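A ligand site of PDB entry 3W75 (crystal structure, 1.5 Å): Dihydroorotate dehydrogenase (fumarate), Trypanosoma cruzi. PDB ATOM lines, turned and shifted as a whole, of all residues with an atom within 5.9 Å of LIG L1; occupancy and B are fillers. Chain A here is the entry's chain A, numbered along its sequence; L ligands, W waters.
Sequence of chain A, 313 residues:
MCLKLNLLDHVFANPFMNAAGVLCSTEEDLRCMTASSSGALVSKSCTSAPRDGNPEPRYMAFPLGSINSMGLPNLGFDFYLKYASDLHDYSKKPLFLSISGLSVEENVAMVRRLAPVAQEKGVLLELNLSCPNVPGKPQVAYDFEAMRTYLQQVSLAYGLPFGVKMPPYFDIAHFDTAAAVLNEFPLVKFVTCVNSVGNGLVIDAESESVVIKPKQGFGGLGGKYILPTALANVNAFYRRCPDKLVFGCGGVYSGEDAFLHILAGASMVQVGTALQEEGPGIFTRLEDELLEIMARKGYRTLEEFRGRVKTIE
A nitrogen (N1) of LG2 L2 sits close to a nitrogen (N2) of LIG L1 (3.4 Å).
O3 of LIG L1 is in hydrogen-bond range of OG of Ser 196. The side-chain amide oxygen (OD1) of Asn 195 sits at hydrogen-bond distance from a nitrogen (N2) of LIG L1. The backbone NH (N) of Leu 72 lies within hydrogen-bond range of an oxygen (O1) of LIG L1, at 2.9 Å. The side-chain amide oxygen (OD1) of Asn 68 is in hydrogen-bond range of a nitrogen (N1) of LIG L1 (2.9 Å). The side-chain amino group (NZ) of Lys 44 is in salt-bridge range of an oxygen (O1) of LIG L1, at 2.9 Å. O4 of LIG L1 is in hydrogen-bond range of ND2 of Asn 128, at 2.9 Å. The backbone NH (N) of Met 70 sits at hydrogen-bond distance from an oxygen (O2) of LIG L1, at 3.0 Å. The backbone NH (N) of Gly 71 lies within hydrogen-bond range of an oxygen (O2) of LIG L1, at 3.1 Å. NZ of Lys 44 is in hydrogen-bond range of O2 of LG2 L2 (2.8 Å). The side-chain amide nitrogen (ND2) of Asn 128 is in hydrogen-bond range of an oxygen (O1) of LG2 L2, at 3.3 Å. N of Ser 45 lies within hydrogen-bond range of O2 of LG2 L2 (3.4 Å). OG of Ser 45 is in hydrogen-bond range of N2 of LG2 L2 (2.7 Å). O3 of LG2 L2 lies within hydrogen-bond range of NZ of Lys 165 (2.9 Å).
The backbone carbonyl oxygen of Cys 131 sits close to an oxygen (O5) of LIG L1. Merely in contact with LIG L1: Asn 54, Ser 69, Pro 73, Ser 130, Pro 132, Asn 133 and Gln 139. Hydrophobic or aromatic side chains within 4 Å of LIG L1: Met 70, Leu 72, Pro 73 and Pro 132.
OG of Ser 196 lies within hydrogen-bond range of OD1 of Asn 195 (3.5 Å). ND2 of Asn 195 is in hydrogen-bond range of OD1 of Asn 128, 3.4 Å away. The backbone NH (N) of Gly 220 sits at hydrogen-bond distance from the backbone carbonyl oxygen (O) of Asn 68 (2.8 Å). The side-chain amide nitrogen (ND2) of Asn 128 lies within hydrogen-bond range of the side-chain hydroxyl (OG) of Ser 45 (3.1 Å). O of Met 70 sits at hydrogen-bond distance from N of Asn 54 (2.9 Å). The backbone carbonyl oxygen (O) of Ser 69 lies within hydrogen-bond range of the side-chain amide nitrogen (ND2) of Asn 54 (3.1 Å). OG of Ser 100 lies within hydrogen-bond range of O of Ser 130, at 2.8 Å. The side-chain amide nitrogen (NE2) of Gln 139 lies close to the side-chain amide nitrogen (ND2) of Asn 133, at 2.6 Å.
Water W1 bridges O2 of LIG L1 (2.8 Å) and O of Asn 68 (3.0 Å).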
ATOM      1  N   LYS A  44       8.324  -1.969  38.647  1.00  0.00           N
ATOM      2  CA  LYS A  44       8.594  -1.616  37.257  1.00  0.00           C
ATOM      3  C   LYS A  44       7.425  -0.787  36.763  1.00  0.00           C
ATOM      4  O   LYS A  44       6.264  -1.122  37.031  1.00  0.00           O
ATOM      5  CB  LYS A  44       8.625  -2.898  36.449  1.00  0.00           C
ATOM      6  CG  LYS A  44       8.650  -2.685  34.983  1.00  0.00           C
ATOM      7  CD  LYS A  44       9.948  -2.044  34.391  1.00  0.00           C
ATOM      8  CE  LYS A  44       9.882  -1.562  32.957  1.00  0.00           C
ATOM      9  NZ  LYS A  44      11.087  -0.806  32.456  1.00  0.00           N
ATOM     10  N   SER A  45       7.645   0.232  35.958  1.00  0.00           N
ATOM     11  CA  SER A  45       6.515   0.966  35.384  1.00  0.00           C
ATOM     12  C   SER A  45       5.664   0.036  34.563  1.00  0.00           C
ATOM     13  O   SER A  45       6.162  -0.757  33.754  1.00  0.00           O
ATOM     14  CB  SER A  45       7.013   2.085  34.488  1.00  0.00           C
ATOM     15  OG  SER A  45       7.681   3.125  35.223  1.00  0.00           O
ATOM     16  N   ASN A  54      11.351  -4.486  24.068  1.00  0.00           N
ATOM     17  CA  ASN A  54      12.136  -4.468  22.863  1.00  0.00           C
ATOM     18  C   ASN A  54      13.021  -5.655  22.737  1.00  0.00           C
ATOM     19  O   ASN A  54      13.313  -6.396  23.671  1.00  0.00           O
ATOM     20  CB  ASN A  54      12.971  -3.129  22.831  1.00  0.00           C
ATOM     21  CG  ASN A  54      12.161  -1.943  22.503  1.00  0.00           C
ATOM     22  OD1 ASN A  54      10.988  -2.034  22.037  1.00  0.00           O
ATOM     23  ND2 ASN A  54      12.691  -0.779  22.763  1.00  0.00           N
ATOM     24  N   ASN A  68      19.989   2.021  27.985  1.00  0.00           N
ATOM     25  CA  ASN A  68      18.852   1.078  27.874  1.00  0.00           C
ATOM     26  C   ASN A  68      17.832   1.604  26.949  1.00  0.00           C
ATOM     27  O   ASN A  68      17.482   2.753  26.879  1.00  0.00           O
ATOM     28  CB  ASN A  68      18.261   0.726  29.211  1.00  0.00           C
ATOM     29  CG  ASN A  68      17.193   1.674  29.657  1.00  0.00           C
ATOM     30  OD1 ASN A  68      16.010   1.568  29.285  1.00  0.00           O
ATOM     31  ND2 ASN A  68      17.550   2.612  30.499  1.00  0.00           N
ATOM     32  N   SER A  69      17.240   0.618  26.223  1.00  0.00           N
ATOM     33  CA  SER A  69      15.988   0.802  25.439  1.00  0.00           C
ATOM     34  C   SER A  69      15.124  -0.394  25.773  1.00  0.00           C
ATOM     35  O   SER A  69      14.861  -1.208  24.878  1.00  0.00           O
ATOM     36  CB  SER A  69      16.284   0.922  23.958  1.00  0.00           C
ATOM     37  OG  SER A  69      15.066   1.186  23.265  1.00  0.00           O
ATOM     38  N   MET A  70      14.716  -0.544  27.009  1.00  0.00           N
ATOM     39  CA  MET A  70      13.964  -1.732  27.409  1.00  0.00           C
ATOM     40  C   MET A  70      12.654  -1.818  26.656  1.00  0.00           C
ATOM     41  O   MET A  70      12.278  -2.995  26.333  1.00  0.00           O
ATOM     42  CB  MET A  70      13.741  -1.798  28.909  1.00  0.00           C
ATOM     43  CG  MET A  70      14.966  -1.652  29.806  1.00  0.00           C
ATOM     44  SD  MET A  70      16.202  -2.868  29.499  1.00  0.00           S
ATOM     45  CE  MET A  70      15.455  -4.207  30.184  1.00  0.00           C
ATOM     46  N   GLY A  71      11.937  -0.761  26.457  1.00  0.00           N
ATOM     47  CA  GLY A  71      10.633  -0.826  25.809  1.00  0.00           C
ATOM     48  C   GLY A  71       9.514  -1.064  26.742  1.00  0.00           C
ATOM     49  O   GLY A  71       8.473  -1.610  26.299  1.00  0.00           O
ATOM     50  N   LEU A  72       9.601  -0.737  28.011  1.00  0.00           N
ATOM     51  CA  LEU A  72       8.565  -0.894  29.004  1.00  0.00           C
ATOM     52  C   LEU A  72       8.129  -2.319  29.104  1.00  0.00           C
ATOM     53  O   LEU A  72       6.881  -2.592  29.193  1.00  0.00           O
ATOM     54  CB  LEU A  72       7.455   0.108  28.668  1.00  0.00           C
ATOM     55  CG  LEU A  72       6.385   0.523  29.565  1.00  0.00           C
ATOM     56  CD1 LEU A  72       6.909   0.860  30.975  1.00  0.00           C
ATOM     57  CD2 LEU A  72       5.682   1.726  28.967  1.00  0.00           C
ATOM     58  N   PRO A  73       9.004  -3.303  29.141  1.00  0.00           N
ATOM     59  CA  PRO A  73       8.573  -4.706  29.379  1.00  0.00           C
ATOM     60  C   PRO A  73       7.968  -4.779  30.786  1.00  0.00           C
ATOM     61  O   PRO A  73       8.615  -4.279  31.738  1.00  0.00           O
ATOM     62  CB  PRO A  73       9.844  -5.561  29.318  1.00  0.00           C
ATOM     63  CG  PRO A  73      10.921  -4.532  29.666  1.00  0.00           C
ATOM     64  CD  PRO A  73      10.491  -3.164  29.205  1.00  0.00           C
ATOM     65  N   SER A 100       3.111   3.839  33.837  1.00  0.00           N
ATOM     66  CA  SER A 100       3.454   4.504  32.618  1.00  0.00           C
ATOM     67  C   SER A 100       2.504   4.073  31.518  1.00  0.00           C
ATOM     68  O   SER A 100       2.891   3.442  30.607  1.00  0.00           O
ATOM     69  CB  SER A 100       4.959   4.320  32.243  1.00  0.00           C
ATOM     70  OG  SER A 100       5.208   5.137  31.140  1.00  0.00           O
ATOM     71  N   ASN A 128       4.975   7.822  36.071  1.00  0.00           N
ATOM     72  CA  ASN A 128       6.092   7.984  35.128  1.00  0.00           C
ATOM     73  C   ASN A 128       5.659   8.714  33.893  1.00  0.00           C
ATOM     74  O   ASN A 128       4.917   8.116  33.095  1.00  0.00           O
ATOM     75  CB  ASN A 128       6.722   6.635  34.797  1.00  0.00           C
ATOM     76  CG  ASN A 128       7.889   6.701  33.834  1.00  0.00           C
ATOM     77  OD1 ASN A 128       8.363   7.774  33.501  1.00  0.00           O
ATOM     78  ND2 ASN A 128       8.340   5.544  33.405  1.00  0.00           N
ATOM     79  N   SER A 130       7.465   9.440  31.282  1.00  0.00           N
ATOM     80  CA  SER A 130       8.227   9.006  30.093  1.00  0.00           C
ATOM     81  C   SER A 130       7.649   7.784  29.481  1.00  0.00           C
ATOM     82  O   SER A 130       7.225   6.898  30.226  1.00  0.00           O
ATOM     83  CB  SER A 130       9.660   8.703  30.505  1.00  0.00           C
ATOM     84  OG  SER A 130      10.372   9.875  31.019  1.00  0.00           O
ATOM     85  N   CYS A 131       7.678   7.693  28.172  1.00  0.00           N
ATOM     86  CA  CYS A 131       7.195   6.504  27.464  1.00  0.00           C
ATOM     87  C   CYS A 131       7.839   6.368  26.118  1.00  0.00           C
ATOM     88  O   CYS A 131       8.453   7.294  25.624  1.00  0.00           O
ATOM     89  CB  CYS A 131       5.667   6.426  27.376  1.00  0.00           C
ATOM     90  SG  CYS A 131       4.887   7.662  26.356  1.00  0.00           S
ATOM     91  N   PRO A 132       7.616   5.190  25.479  1.00  0.00           N
ATOM     92  CA  PRO A 132       8.263   5.034  24.156  1.00  0.00           C
ATOM     93  C   PRO A 132       7.888   6.141  23.191  1.00  0.00           C
ATOM     94  O   PRO A 132       6.725   6.577  23.234  1.00  0.00           O
ATOM     95  CB  PRO A 132       7.780   3.628  23.768  1.00  0.00           C
ATOM     96  CG  PRO A 132       7.576   2.876  25.033  1.00  0.00           C
ATOM     97  CD  PRO A 132       7.001   3.939  25.993  1.00  0.00           C
ATOM     98  N   ASN A 133       8.799   6.568  22.347  1.00  0.00           N
ATOM     99  CA  ASN A 133       8.577   7.690  21.478  1.00  0.00           C
ATOM    100  C   ASN A 133       7.539   7.359  20.403  1.00  0.00           C
ATOM    101  O   ASN A 133       7.438   6.212  19.959  1.00  0.00           O
ATOM    102  CB  ASN A 133       9.857   8.047  20.768  1.00  0.00           C
ATOM    103  CG  ASN A 133      10.863   8.556  21.725  1.00  0.00           C
ATOM    104  OD1 ASN A 133      12.023   8.038  21.872  1.00  0.00           O
ATOM    105  ND2 ASN A 133      10.400   9.565  22.454  1.00  0.00           N
ATOM    106  N   GLN A 139       8.129  13.870  24.232  1.00  0.00           N
ATOM    107  CA  GLN A 139       7.816  13.291  25.498  1.00  0.00           C
ATOM    108  C   GLN A 139       6.904  14.235  26.306  1.00  0.00           C
ATOM    109  O   GLN A 139       7.030  15.469  26.271  1.00  0.00           O
ATOM    110  CB  GLN A 139       9.138  13.070  26.266  1.00  0.00           C
ATOM    111  CG  GLN A 139      10.000  11.941  25.680  1.00  0.00           C
ATOM    112  CD  GLN A 139       9.405  10.625  25.906  1.00  0.00           C
ATOM    113  OE1 GLN A 139       9.010  10.268  27.024  1.00  0.00           O
ATOM    114  NE2 GLN A 139       9.296   9.846  24.832  1.00  0.00           N
ATOM    115  N   LYS A 165       7.538  10.986  38.288  1.00  0.00           N
ATOM    116  CA  LYS A 165       8.904  10.717  37.804  1.00  0.00           C
ATOM    117  C   LYS A 165       9.128  11.564  36.537  1.00  0.00           C
ATOM    118  O   LYS A 165       8.444  11.431  35.564  1.00  0.00           O
ATOM    119  CB  LYS A 165       9.109   9.274  37.572  1.00  0.00           C
ATOM    120  CG  LYS A 165      10.460   8.825  36.960  1.00  0.00           C
ATOM    121  CD  LYS A 165      11.430   8.727  38.043  1.00  0.00           C
ATOM    122  CE  LYS A 165      12.772   8.132  37.578  1.00  0.00           C
ATOM    123  NZ  LYS A 165      12.717   6.656  37.452  1.00  0.00           N
ATOM    124  N   ASN A 195      14.638  10.535  35.630  1.00  0.00           N
ATOM    125  CA  ASN A 195      14.739   9.419  34.706  1.00  0.00           C
ATOM    126  C   ASN A 195      16.060   9.483  33.961  1.00  0.00           C
ATOM    127  O   ASN A 195      16.874  10.427  34.085  1.00  0.00           O
ATOM    128  CB  ASN A 195      13.513   9.420  33.780  1.00  0.00           C
ATOM    129  CG  ASN A 195      13.049   8.023  33.481  1.00  0.00           C
ATOM    130  OD1 ASN A 195      13.845   7.176  33.062  1.00  0.00           O
ATOM    131  ND2 ASN A 195      11.743   7.834  33.530  1.00  0.00           N
ATOM    132  N   SER A 196      16.332   8.457  33.195  1.00  0.00           N
ATOM    133  CA  SER A 196      17.579   8.413  32.391  1.00  0.00           C
ATOM    134  C   SER A 196      17.624   9.586  31.421  1.00  0.00           C
ATOM    135  O   SER A 196      16.591  10.188  31.054  1.00  0.00           O
ATOM    136  CB  SER A 196      17.678   7.047  31.716  1.00  0.00           C
ATOM    137  OG  SER A 196      16.563   6.827  30.896  1.00  0.00           O
ATOM    138  N   ASN A 199      18.133   9.417  24.935  1.00  0.00           N
ATOM    139  CA  ASN A 199      18.694   9.300  23.608  1.00  0.00           C
ATOM    140  C   ASN A 199      20.202   9.582  23.554  1.00  0.00           C
ATOM    141  O   ASN A 199      20.704  10.310  22.695  1.00  0.00           O
ATOM    142  CB  ASN A 199      17.931  10.172  22.633  1.00  0.00           C
ATOM    143  CG  ASN A 199      16.583   9.656  22.414  1.00  0.00           C
ATOM    144  OD1 ASN A 199      16.409   8.572  21.876  1.00  0.00           O
ATOM    145  ND2 ASN A 199      15.618  10.350  22.936  1.00  0.00           N
ATOM    146  N   LYS A 215      16.191   0.857  18.222  1.00  0.00           N
ATOM    147  CA  LYS A 215      16.299   2.276  17.955  1.00  0.00           C
ATOM    148  C   LYS A 215      17.680   2.689  17.499  1.00  0.00           C
ATOM    149  O   LYS A 215      18.196   3.719  17.871  1.00  0.00           O
ATOM    150  CB  LYS A 215      15.821   3.090  19.166  1.00  0.00           C
ATOM    151  CG  LYS A 215      14.404   2.746  19.568  1.00  0.00           C
ATOM    152  CD  LYS A 215      13.414   3.062  18.511  1.00  0.00           C
ATOM    153  CE  LYS A 215      12.680   4.360  18.754  1.00  0.00           C
ATOM    154  NZ  LYS A 215      11.359   4.137  18.014  1.00  0.00           N
ATOM    155  N   GLY A 220      18.339   5.465  26.879  1.00  0.00           N
ATOM    156  CA  GLY A 220      18.511   6.355  27.984  1.00  0.00           C
ATOM    157  C   GLY A 220      19.774   6.003  28.743  1.00  0.00           C
ATOM    158  O   GLY A 220      20.108   4.819  28.980  1.00  0.00           O
HETATM  159  O1  LIG L   1      11.385   0.527  29.867  1.00  0.00           O
HETATM  160  C1  LIG L   1      12.246   1.410  29.518  1.00  0.00           C
HETATM  161  O2  LIG L   1      12.918   1.412  28.446  1.00  0.00           O
HETATM  162  C2  LIG L   1      12.411   2.621  30.345  1.00  0.00           C
HETATM  163  N1  LIG L   1      13.779   3.007  30.481  1.00  0.00           N
HETATM  164  C3  LIG L   1      14.117   4.133  31.157  1.00  0.00           C
HETATM  165  O3  LIG L   1      15.347   4.431  31.295  1.00  0.00           O
HETATM  166  N2  LIG L   1      13.142   4.871  31.735  1.00  0.00           N
HETATM  167  C4  LIG L   1      11.797   4.545  31.628  1.00  0.00           C
HETATM  168  O4  LIG L   1      10.995   5.335  32.160  1.00  0.00           O
HETATM  169  C5  LIG L   1      11.433   3.372  30.922  1.00  0.00           C
HETATM  170  C6  LIG L   1       9.958   3.055  30.755  1.00  0.00           C
HETATM  171  C7  LIG L   1       9.260   4.100  29.863  1.00  0.00           C
HETATM  172  C8  LIG L   1       9.906   4.257  28.596  1.00  0.00           C
HETATM  173  C9  LIG L   1      10.299   3.236  27.721  1.00  0.00           C
HETATM  174  C10 LIG L   1      10.388   5.499  28.153  1.00  0.00           C
HETATM  175  C11 LIG L   1      11.023   5.715  26.965  1.00  0.00           C
HETATM  176  O5  LIG L   1      11.430   7.053  26.752  1.00  0.00           O
HETATM  177  C12 LIG L   1      11.886   7.248  25.522  1.00  0.00           C
HETATM  178  C13 LIG L   1      11.394   4.696  26.147  1.00  0.00           C
HETATM  179  C14 LIG L   1      10.979   3.421  26.530  1.00  0.00           C
HETATM  180  O6  LIG L   1      11.284   2.288  25.801  1.00  0.00           O
HETATM  181  C15 LIG L   1      12.304   2.433  24.799  1.00  0.00           C
HETATM  182  N1  LG2 L   2      12.480   4.533  35.065  1.00  0.00           N
HETATM  183  C1  LG2 L   2      11.157   4.486  35.266  1.00  0.00           C
HETATM  184  O1  LG2 L   2      10.592   5.420  35.871  1.00  0.00           O
HETATM  185  N2  LG2 L   2      10.407   3.354  34.962  1.00  0.00           N
HETATM  186  C2  LG2 L   2      10.981   2.342  34.407  1.00  0.00           C
HETATM  187  O2  LG2 L   2      10.298   1.286  34.165  1.00  0.00           O
HETATM  188  C3  LG2 L   2      12.367   2.311  34.149  1.00  0.00           C
HETATM  189  N3  LG2 L   2      13.027   1.244  33.574  1.00  0.00           N
HETATM  190  C4  LG2 L   2      14.394   1.219  33.641  1.00  0.00           C
HETATM  191  C5  LG2 L   2      15.047   0.097  33.246  1.00  0.00           C
HETATM  192  C6  LG2 L   2      16.436   0.040  33.275  1.00  0.00           C
HETATM  193  C7  LG2 L   2      17.157  -1.275  32.890  1.00  0.00           C
HETATM  194  C8  LG2 L   2      17.208   1.145  33.665  1.00  0.00           C
HETATM  195  C9  LG2 L   2      18.695   1.096  33.675  1.00  0.00           C
HETATM  196  C10 LG2 L   2      16.523   2.270  34.024  1.00  0.00           C
HETATM  197  C11 LG2 L   2      15.150   2.355  34.027  1.00  0.00           C
HETATM  198  N4  LG2 L   2      14.488   3.504  34.421  1.00  0.00           N
HETATM  199  C12 LG2 L   2      13.114   3.490  34.558  1.00  0.00           C
HETATM  200  C13 LG2 L   2      15.194   4.721  34.804  1.00  0.00           C
HETATM  201  C14 LG2 L   2      15.733   4.581  36.223  1.00  0.00           C
HETATM  202  O3  LG2 L   2      14.633   4.497  37.149  1.00  0.00           O
HETATM  203  C15 LG2 L   2      16.611   5.771  36.629  1.00  0.00           C
HETATM  204  O4  LG2 L   2      15.746   6.950  36.574  1.00  0.00           O
HETATM  205  C16 LG2 L   2      17.819   6.001  35.737  1.00  0.00           C
HETATM  206  O5  LG2 L   2      18.425   4.724  35.357  1.00  0.00           O
HETATM  207  C17 LG2 L   2      18.908   6.881  36.353  1.00  0.00           C
HETATM  208  O6  LG2 L   2      19.313   6.395  37.613  1.00  0.00           O
HETATM  209  P1  LG2 L   2      20.800   5.695  37.661  1.00  0.00           P
HETATM  210  O7  LG2 L   2      20.923   5.267  39.061  1.00  0.00           O
HETATM  211  O8  LG2 L   2      21.811   6.712  37.254  1.00  0.00           O
HETATM  212  O9  LG2 L   2      20.760   4.518  36.697  1.00  0.00           O
HETATM  213  O   HOH W   1      14.604   3.389  27.355  1.00  0.00           O
HETATM  214  O   HOH W   2      11.011   1.515  21.691  1.00  0.00           O
